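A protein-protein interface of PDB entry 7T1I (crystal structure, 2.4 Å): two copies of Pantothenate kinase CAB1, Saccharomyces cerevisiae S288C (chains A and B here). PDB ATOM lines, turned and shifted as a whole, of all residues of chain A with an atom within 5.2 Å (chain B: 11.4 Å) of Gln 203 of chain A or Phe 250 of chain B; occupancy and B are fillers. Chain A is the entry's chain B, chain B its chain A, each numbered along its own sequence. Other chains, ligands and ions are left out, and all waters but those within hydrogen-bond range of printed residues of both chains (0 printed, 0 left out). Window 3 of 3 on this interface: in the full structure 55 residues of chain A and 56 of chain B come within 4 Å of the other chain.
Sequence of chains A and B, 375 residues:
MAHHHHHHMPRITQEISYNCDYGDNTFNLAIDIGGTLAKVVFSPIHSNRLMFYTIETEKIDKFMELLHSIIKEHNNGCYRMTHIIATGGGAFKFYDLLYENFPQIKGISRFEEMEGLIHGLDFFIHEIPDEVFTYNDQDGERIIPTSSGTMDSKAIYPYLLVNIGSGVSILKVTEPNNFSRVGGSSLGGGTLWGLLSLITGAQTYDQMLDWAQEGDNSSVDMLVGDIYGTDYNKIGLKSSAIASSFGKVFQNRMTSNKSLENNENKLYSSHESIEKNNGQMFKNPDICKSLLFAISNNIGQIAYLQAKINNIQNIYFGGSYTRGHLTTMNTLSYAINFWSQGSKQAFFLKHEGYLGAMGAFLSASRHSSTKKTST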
ATOM      1  N   TRP A 193      15.848 -15.302 -18.502  1.00  0.00           N
ATOM      2  CA  TRP A 193      14.856 -16.313 -18.190  1.00  0.00           C
ATOM      3  C   TRP A 193      15.083 -16.819 -16.763  1.00  0.00           C
ATOM      4  O   TRP A 193      14.141 -16.874 -15.980  1.00  0.00           O
ATOM      5  CB  TRP A 193      14.799 -17.421 -19.270  1.00  0.00           C
ATOM      6  CG  TRP A 193      14.827 -16.928 -20.695  1.00  0.00           C
ATOM      7  CD1 TRP A 193      14.208 -15.807 -21.183  1.00  0.00           C
ATOM      8  CD2 TRP A 193      15.519 -17.515 -21.831  1.00  0.00           C
ATOM      9  NE1 TRP A 193      14.461 -15.656 -22.525  1.00  0.00           N
ATOM     10  CE2 TRP A 193      15.268 -16.681 -22.954  1.00  0.00           C
ATOM     11  CE3 TRP A 193      16.327 -18.655 -22.026  1.00  0.00           C
ATOM     12  CZ2 TRP A 193      15.784 -16.956 -24.229  1.00  0.00           C
ATOM     13  CZ3 TRP A 193      16.855 -18.914 -23.280  1.00  0.00           C
ATOM     14  CH2 TRP A 193      16.584 -18.075 -24.368  1.00  0.00           C
ATOM     15  N   GLY A 194      16.344 -17.088 -16.403  1.00  0.00           N
ATOM     16  CA  GLY A 194      16.725 -17.492 -15.057  1.00  0.00           C
ATOM     17  C   GLY A 194      16.289 -16.516 -13.949  1.00  0.00           C
ATOM     18  O   GLY A 194      15.502 -16.872 -13.073  1.00  0.00           O
ATOM     19  N   SER A 197      12.486 -15.861 -13.844  1.00  0.00           N
ATOM     20  CA  SER A 197      11.648 -17.008 -13.568  1.00  0.00           C
ATOM     21  C   SER A 197      11.644 -17.299 -12.072  1.00  0.00           C
ATOM     22  O   SER A 197      10.605 -17.585 -11.489  1.00  0.00           O
ATOM     23  CB  SER A 197      12.103 -18.194 -14.345  1.00  0.00           C
ATOM     24  OG  SER A 197      11.086 -19.172 -14.310  1.00  0.00           O
ATOM     25  N   GLY A 201       8.188 -15.537 -11.197  1.00  0.00           N
ATOM     26  CA  GLY A 201       7.408 -16.764 -11.276  1.00  0.00           C
ATOM     27  C   GLY A 201       6.864 -16.959 -12.690  1.00  0.00           C
ATOM     28  O   GLY A 201       6.115 -17.897 -12.945  1.00  0.00           O
ATOM     29  N   ALA A 202       7.255 -16.062 -13.607  1.00  0.00           N
ATOM     30  CA  ALA A 202       6.865 -16.152 -15.008  1.00  0.00           C
ATOM     31  C   ALA A 202       7.062 -17.577 -15.539  1.00  0.00           C
ATOM     32  O   ALA A 202       8.065 -18.234 -15.248  1.00  0.00           O
ATOM     33  CB  ALA A 202       7.623 -15.130 -15.820  1.00  0.00           C
ATOM     34  N   GLN A 203       6.076 -18.044 -16.318  1.00  0.00           N
ATOM     35  CA  GLN A 203       6.029 -19.421 -16.793  1.00  0.00           C
ATOM     36  C   GLN A 203       6.875 -19.569 -18.052  1.00  0.00           C
ATOM     37  O   GLN A 203       7.584 -20.560 -18.191  1.00  0.00           O
ATOM     38  CB  GLN A 203       4.594 -19.855 -17.120  1.00  0.00           C
ATOM     39  CG  GLN A 203       3.585 -19.602 -16.005  1.00  0.00           C
ATOM     40  CD  GLN A 203       3.805 -20.457 -14.778  1.00  0.00           C
ATOM     41  OE1 GLN A 203       4.879 -21.020 -14.566  1.00  0.00           O
ATOM     42  NE2 GLN A 203       2.781 -20.555 -13.947  1.00  0.00           N
ATOM     43  N   THR A 204       6.773 -18.571 -18.943  1.00  0.00           N
ATOM     44  CA  THR A 204       7.288 -18.617 -20.304  1.00  0.00           C
ATOM     45  C   THR A 204       8.025 -17.320 -20.632  1.00  0.00           C
ATOM     46  O   THR A 204       7.761 -16.287 -20.018  1.00  0.00           O
ATOM     47  CB  THR A 204       6.145 -18.744 -21.323  1.00  0.00           C
ATOM     48  OG1 THR A 204       5.224 -17.658 -21.170  1.00  0.00           O
ATOM     49  CG2 THR A 204       5.438 -20.084 -21.285  1.00  0.00           C
ATOM     50  N   TYR A 205       8.913 -17.377 -21.637  1.00  0.00           N
ATOM     51  CA  TYR A 205       9.548 -16.169 -22.149  1.00  0.00           C
ATOM     52  C   TYR A 205       8.472 -15.203 -22.669  1.00  0.00           C
ATOM     53  O   TYR A 205       8.646 -13.983 -22.615  1.00  0.00           O
ATOM     54  CB  TYR A 205      10.719 -16.514 -23.087  1.00  0.00           C
ATOM     55  CG  TYR A 205      11.462 -15.362 -23.737  1.00  0.00           C
ATOM     56  CD1 TYR A 205      11.805 -14.215 -23.027  1.00  0.00           C
ATOM     57  CD2 TYR A 205      11.865 -15.428 -25.066  1.00  0.00           C
ATOM     58  CE1 TYR A 205      12.496 -13.165 -23.620  1.00  0.00           C
ATOM     59  CE2 TYR A 205      12.564 -14.392 -25.676  1.00  0.00           C
ATOM     60  CZ  TYR A 205      12.883 -13.252 -24.949  1.00  0.00           C
ATOM     61  OH  TYR A 205      13.565 -12.217 -25.527  1.00  0.00           O
ATOM     62  N   GLN A 207       5.446 -14.706 -21.333  1.00  0.00           N
ATOM     63  CA  GLN A 207       4.747 -14.063 -20.232  1.00  0.00           C
ATOM     64  C   GLN A 207       5.680 -13.141 -19.432  1.00  0.00           C
ATOM     65  O   GLN A 207       5.230 -12.442 -18.523  1.00  0.00           O
ATOM     66  CB  GLN A 207       4.034 -15.122 -19.386  1.00  0.00           C
ATOM     67  CG  GLN A 207       2.660 -14.679 -18.904  1.00  0.00           C
ATOM     68  CD  GLN A 207       2.556 -14.735 -17.398  1.00  0.00           C
ATOM     69  OE1 GLN A 207       3.214 -15.540 -16.733  1.00  0.00           O
ATOM     70  NE2 GLN A 207       1.725 -13.861 -16.848  1.00  0.00           N
ATOM     71  N   MET A 208       6.982 -13.149 -19.757  1.00  0.00           N
ATOM     72  CA  MET A 208       7.912 -12.159 -19.235  1.00  0.00           C
ATOM     73  C   MET A 208       7.717 -10.849 -19.988  1.00  0.00           C
ATOM     74  O   MET A 208       7.792  -9.776 -19.394  1.00  0.00           O
ATOM     75  CB  MET A 208       9.367 -12.599 -19.412  1.00  0.00           C
ATOM     76  CG  MET A 208       9.826 -13.568 -18.356  1.00  0.00           C
ATOM     77  SD  MET A 208      11.261 -14.513 -18.913  1.00  0.00           S
ATOM     78  CE  MET A 208      11.040 -16.002 -17.937  1.00  0.00           C
ATOM     79  N   ILE B 199      16.879 -11.827  -3.962  1.00  0.00           N
ATOM     80  CA  ILE B 199      16.778 -13.258  -4.234  1.00  0.00           C
ATOM     81  C   ILE B 199      17.111 -14.049  -2.971  1.00  0.00           C
ATOM     82  O   ILE B 199      16.354 -14.931  -2.594  1.00  0.00           O
ATOM     83  CB  ILE B 199      17.631 -13.711  -5.443  1.00  0.00           C
ATOM     84  CG1 ILE B 199      17.077 -13.196  -6.770  1.00  0.00           C
ATOM     85  CG2 ILE B 199      17.799 -15.229  -5.485  1.00  0.00           C
ATOM     86  CD1 ILE B 199      18.076 -13.288  -7.895  1.00  0.00           C
ATOM     87  N   SER B 219      26.245 -24.791  -9.948  1.00  0.00           N
ATOM     88  CA  SER B 219      24.892 -25.239  -9.660  1.00  0.00           C
ATOM     89  C   SER B 219      23.859 -24.466 -10.491  1.00  0.00           C
ATOM     90  O   SER B 219      22.856 -25.038 -10.912  1.00  0.00           O
ATOM     91  CB  SER B 219      24.632 -25.232  -8.160  1.00  0.00           C
ATOM     92  OG  SER B 219      23.465 -24.496  -7.787  1.00  0.00           O
ATOM     93  N   VAL B 220      24.100 -23.169 -10.761  1.00  0.00           N
ATOM     94  CA  VAL B 220      23.072 -22.364 -11.416  1.00  0.00           C
ATOM     95  C   VAL B 220      23.491 -21.957 -12.823  1.00  0.00           C
ATOM     96  O   VAL B 220      22.633 -21.596 -13.623  1.00  0.00           O
ATOM     97  CB  VAL B 220      22.659 -21.132 -10.587  1.00  0.00           C
ATOM     98  CG1 VAL B 220      21.784 -21.529  -9.408  1.00  0.00           C
ATOM     99  CG2 VAL B 220      23.861 -20.300 -10.152  1.00  0.00           C
ATOM    100  N   ASP B 221      24.791 -21.997 -13.112  1.00  0.00           N
ATOM    101  CA  ASP B 221      25.329 -21.532 -14.388  1.00  0.00           C
ATOM    102  C   ASP B 221      25.544 -22.704 -15.355  1.00  0.00           C
ATOM    103  O   ASP B 221      25.997 -23.769 -14.954  1.00  0.00           O
ATOM    104  CB  ASP B 221      26.702 -20.874 -14.187  1.00  0.00           C
ATOM    105  CG  ASP B 221      26.677 -19.541 -13.446  1.00  0.00           C
ATOM    106  OD1 ASP B 221      25.592 -18.875 -13.410  1.00  0.00           O
ATOM    107  OD2 ASP B 221      27.743 -19.170 -12.912  1.00  0.00           O
ATOM    108  N   MET B 222      25.309 -22.478 -16.653  1.00  0.00           N
ATOM    109  CA  MET B 222      25.817 -23.382 -17.673  1.00  0.00           C
ATOM    110  C   MET B 222      27.290 -23.082 -17.976  1.00  0.00           C
ATOM    111  O   MET B 222      27.635 -21.963 -18.382  1.00  0.00           O
ATOM    112  CB  MET B 222      24.996 -23.246 -18.956  1.00  0.00           C
ATOM    113  CG  MET B 222      23.558 -23.684 -18.795  1.00  0.00           C
ATOM    114  SD  MET B 222      22.484 -23.406 -20.242  1.00  0.00           S
ATOM    115  CE  MET B 222      23.491 -24.078 -21.571  1.00  0.00           C
ATOM    116  N   SER B 244      26.647 -19.388 -19.673  1.00  0.00           N
ATOM    117  CA  SER B 244      25.375 -18.745 -19.391  1.00  0.00           C
ATOM    118  C   SER B 244      25.158 -18.621 -17.892  1.00  0.00           C
ATOM    119  O   SER B 244      24.848 -19.614 -17.231  1.00  0.00           O
ATOM    120  CB  SER B 244      24.229 -19.492 -19.992  1.00  0.00           C
ATOM    121  OG  SER B 244      23.064 -18.711 -19.796  1.00  0.00           O
ATOM    122  N   SER B 245      25.281 -17.386 -17.392  1.00  0.00           N
ATOM    123  CA  SER B 245      25.095 -17.089 -15.982  1.00  0.00           C
ATOM    124  C   SER B 245      23.632 -17.351 -15.641  1.00  0.00           C
ATOM    125  O   SER B 245      22.750 -16.849 -16.336  1.00  0.00           O
ATOM    126  CB  SER B 245      25.485 -15.661 -15.713  1.00  0.00           C
ATOM    127  OG  SER B 245      26.882 -15.545 -15.515  1.00  0.00           O
ATOM    128  N   PHE B 246      23.376 -18.158 -14.600  1.00  0.00           N
ATOM    129  CA  PHE B 246      22.012 -18.515 -14.227  1.00  0.00           C
ATOM    130  C   PHE B 246      21.324 -19.328 -15.325  1.00  0.00           C
ATOM    131  O   PHE B 246      20.094 -19.425 -15.333  1.00  0.00           O
ATOM    132  CB  PHE B 246      21.181 -17.271 -13.882  1.00  0.00           C
ATOM    133  CG  PHE B 246      20.821 -17.168 -12.423  1.00  0.00           C
ATOM    134  CD1 PHE B 246      21.809 -17.029 -11.455  1.00  0.00           C
ATOM    135  CD2 PHE B 246      19.495 -17.212 -12.010  1.00  0.00           C
ATOM    136  CE1 PHE B 246      21.479 -16.972 -10.108  1.00  0.00           C
ATOM    137  CE2 PHE B 246      19.162 -17.147 -10.659  1.00  0.00           C
ATOM    138  CZ  PHE B 246      20.157 -17.018  -9.713  1.00  0.00           C
ATOM    139  N   GLY B 247      22.119 -19.890 -16.248  1.00  0.00           N
ATOM    140  CA  GLY B 247      21.623 -20.620 -17.405  1.00  0.00           C
ATOM    141  C   GLY B 247      20.862 -21.901 -17.046  1.00  0.00           C
ATOM    142  O   GLY B 247      19.993 -22.324 -17.797  1.00  0.00           O
ATOM    143  N   LYS B 248      21.175 -22.508 -15.896  1.00  0.00           N
ATOM    144  CA  LYS B 248      20.535 -23.745 -15.457  1.00  0.00           C
ATOM    145  C   LYS B 248      19.156 -23.519 -14.823  1.00  0.00           C
ATOM    146  O   LYS B 248      18.399 -24.474 -14.683  1.00  0.00           O
ATOM    147  CB  LYS B 248      21.461 -24.533 -14.523  1.00  0.00           C
ATOM    148  CG  LYS B 248      22.543 -25.338 -15.233  1.00  0.00           C
ATOM    149  CD  LYS B 248      23.522 -26.086 -14.344  1.00  0.00           C
ATOM    150  CE  LYS B 248      24.519 -26.872 -15.173  1.00  0.00           C
ATOM    151  NZ  LYS B 248      25.885 -26.893 -14.592  1.00  0.00           N
ATOM    152  N   VAL B 249      18.784 -22.282 -14.460  1.00  0.00           N
ATOM    153  CA  VAL B 249      17.620 -22.144 -13.590  1.00  0.00           C
ATOM    154  C   VAL B 249      16.278 -22.085 -14.327  1.00  0.00           C
ATOM    155  O   VAL B 249      15.299 -22.629 -13.816  1.00  0.00           O
ATOM    156  CB  VAL B 249      17.767 -21.129 -12.438  1.00  0.00           C
ATOM    157  CG1 VAL B 249      19.159 -20.541 -12.328  1.00  0.00           C
ATOM    158  CG2 VAL B 249      16.665 -20.080 -12.399  1.00  0.00           C
ATOM    159  N   PHE B 250      16.197 -21.459 -15.511  1.00  0.00           N
ATOM    160  CA  PHE B 250      14.940 -21.561 -16.257  1.00  0.00           C
ATOM    161  C   PHE B 250      14.806 -22.986 -16.790  1.00  0.00           C
ATOM    162  O   PHE B 250      13.698 -23.516 -16.923  1.00  0.00           O
ATOM    163  CB  PHE B 250      14.805 -20.494 -17.356  1.00  0.00           C
ATOM    164  CG  PHE B 250      13.419 -20.321 -17.945  1.00  0.00           C
ATOM    165  CD1 PHE B 250      12.360 -19.865 -17.177  1.00  0.00           C
ATOM    166  CD2 PHE B 250      13.168 -20.591 -19.284  1.00  0.00           C
ATOM    167  CE1 PHE B 250      11.095 -19.696 -17.720  1.00  0.00           C
ATOM    168  CE2 PHE B 250      11.902 -20.418 -19.828  1.00  0.00           C
ATOM    169  CZ  PHE B 250      10.864 -19.972 -19.045  1.00  0.00           C
ATOM    170  N   GLN B 251      15.983 -23.575 -17.041  1.00  0.00           N
ATOM    171  CA  GLN B 251      16.205 -24.929 -17.519  1.00  0.00           C
ATOM    172  C   GLN B 251      16.075 -25.921 -16.358  1.00  0.00           C
ATOM    173  O   GLN B 251      16.619 -27.025 -16.412  1.00  0.00           O
ATOM    174  CB  GLN B 251      17.612 -24.966 -18.115  1.00  0.00           C
ATOM    175  CG  GLN B 251      17.710 -25.749 -19.408  1.00  0.00           C
ATOM    176  CD  GLN B 251      19.060 -26.407 -19.563  1.00  0.00           C
ATOM    177  OE1 GLN B 251      20.062 -25.986 -18.974  1.00  0.00           O
ATOM    178  NE2 GLN B 251      19.087 -27.459 -20.368  1.00  0.00           N
ATOM    179  N   ASN B 252      15.388 -25.486 -15.290  1.00  0.00           N
ATOM    180  CA  ASN B 252      14.905 -26.346 -14.220  1.00  0.00           C
ATOM    181  C   ASN B 252      13.379 -26.188 -14.141  1.00  0.00           C
ATOM    182  O   ASN B 252      12.710 -26.667 -15.098  1.00  0.00           O
ATOM    183  CB  ASN B 252      15.561 -26.035 -12.866  1.00  0.00           C
ATOM    184  CG  ASN B 252      14.964 -26.822 -11.713  1.00  0.00           C
ATOM    185  OD1 ASN B 252      14.901 -28.047 -11.769  1.00  0.00           O
ATOM    186  ND2 ASN B 252      14.524 -26.145 -10.662  1.00  0.00           N
ATOM    187  N   GLY B 279       9.921 -19.928  -3.879  1.00  0.00           N
ATOM    188  CA  GLY B 279      10.433 -20.109  -5.229  1.00  0.00           C
ATOM    189  C   GLY B 279      11.716 -20.945  -5.261  1.00  0.00           C
ATOM    190  O   GLY B 279      11.901 -21.741  -6.182  1.00  0.00           O
ATOM    191  N   MET B 281      14.714 -23.386  -5.146  1.00  0.00           N
ATOM    192  CA  MET B 281      15.313 -24.706  -5.055  1.00  0.00           C
ATOM    193  C   MET B 281      16.824 -24.569  -5.283  1.00  0.00           C
ATOM    194  O   MET B 281      17.467 -25.524  -5.719  1.00  0.00           O
ATOM    195  CB  MET B 281      14.715 -25.654  -6.104  1.00  0.00           C
ATOM    196  CG  MET B 281      13.228 -25.951  -5.931  1.00  0.00           C
ATOM    197  SD  MET B 281      12.112 -25.000  -7.015  1.00  0.00           S
ATOM    198  CE  MET B 281      12.371 -25.788  -8.607  1.00  0.00           C
ATOM    199  N   PHE B 282      17.392 -23.382  -4.984  1.00  0.00           N
ATOM    200  CA  PHE B 282      18.793 -23.092  -5.287  1.00  0.00           C
ATOM    201  C   PHE B 282      19.540 -22.558  -4.073  1.00  0.00           C
ATOM    202  O   PHE B 282      18.996 -21.782  -3.299  1.00  0.00           O
ATOM    203  CB  PHE B 282      18.920 -22.121  -6.462  1.00  0.00           C
ATOM    204  CG  PHE B 282      18.161 -22.564  -7.686  1.00  0.00           C
ATOM    205  CD1 PHE B 282      18.728 -23.460  -8.583  1.00  0.00           C
ATOM    206  CD2 PHE B 282      16.862 -22.111  -7.917  1.00  0.00           C
ATOM    207  CE1 PHE B 282      18.020 -23.877  -9.702  1.00  0.00           C
ATOM    208  CE2 PHE B 282      16.147 -22.538  -9.029  1.00  0.00           C
ATOM    209  CZ  PHE B 282      16.736 -23.413  -9.921  1.00  0.00           C
ATOM    210  N   ILE B 287      24.079 -18.895  -5.750  1.00  0.00           N
ATOM    211  CA  ILE B 287      23.507 -17.754  -6.428  1.00  0.00           C
ATOM    212  C   ILE B 287      24.464 -16.570  -6.305  1.00  0.00           C
ATOM    213  O   ILE B 287      24.720 -15.909  -7.304  1.00  0.00           O
ATOM    214  CB  ILE B 287      22.077 -17.475  -5.941  1.00  0.00           C
ATOM    215  CG1 ILE B 287      21.132 -18.571  -6.456  1.00  0.00           C
ATOM    216  CG2 ILE B 287      21.608 -16.095  -6.381  1.00  0.00           C
ATOM    217  CD1 ILE B 287      19.927 -18.806  -5.568  1.00  0.00           C
ATOM    218  N   SER B 290      27.483 -16.887  -8.519  1.00  0.00           N
ATOM    219  CA  SER B 290      27.147 -16.789  -9.929  1.00  0.00           C
ATOM    220  C   SER B 290      27.043 -15.314 -10.297  1.00  0.00           C
ATOM    221  O   SER B 290      27.660 -14.855 -11.257  1.00  0.00           O
ATOM    222  CB  SER B 290      25.878 -17.567 -10.208  1.00  0.00           C
ATOM    223  OG  SER B 290      25.170 -17.079 -11.327  1.00  0.00           O
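The backbone NH (N) of Phe 246 of chain B lies within hydrogen-bond range of the side-chain carboxylate (OD1) of Asp 221 of chain B.
OG of Ser 197 of chain A lies within hydrogen-bond range of O of Ala 202 of chain A (3.3 Å).
CB of Trp 193 of chain A touches CG of Phe 250 of chain B, 3.5 Å away.
Phe 246 of chain B touches Gly 194 of chain A (CD2 to C, 3.8 Å).
Gly 194 of chain A touches Val 249 of chain B.
Phe 250 of chain B touches Gly 194 of chain A (CB to N, 3.9 Å).
Phe 250 of chain B touches Ser 197 of chain A.
Phe 250 of chain B touches Gln 203 of chain A.
Phe 250 of chain B touches Met 208 of chain A (CE1 to CE, 3.7 Å).
Gln 203 of chain A touches just one residue of chain B: Phe 250.
Phe 250 of chain B touches just these residues of chain A: Trp 193 (3.5 Å), Gly 194 (3.9 Å), Ser 197 (3.2 Å), Gln 203 (3.4 Å) and Met 208 (3.7 Å).
Of the printed residues of chain B, Ser 197 of chain A touches Phe 250 (3.2 Å).
No residue of chain B comes within 4 Å of Gly 201 of chain A.
No residue of chain B comes within 4 Å of Ala 202 of chain A.
No residue of chain B comes within 4 Å of Thr 204 of chain A.
Gln 207 of chain A touches none of the printed residues of chain B.
Of the printed residues of chain B, Met 208 of chain A touches Phe 250.
Of the printed residues of chain A, Val 249 of chain B touches Gly 194.
The nearest residue of chain A that does not touch Phe 250 of chain B is Thr 204 of chain A (4.03 Å).
The nearest printed residue of chain A that does not touch Phe 246 of chain B is Trp 193 of chain A (5.8 Å).
Printed residues of chain A that touch a printed residue of chain B: Trp 193, Gly 194, Ser 197, Gln 203 and Met 208.
Hydrophobic or aromatic side chains of chain A that line the printed part of chain B: Trp 193 and Met 208.
Of the 19 printed residues of chain B, 3 touch a printed residue of chain A.
No position is printed for both chains.
Of the 7 pairs that touch across the chains among the printed residues, none has its exchanged pair printed and touching as well.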
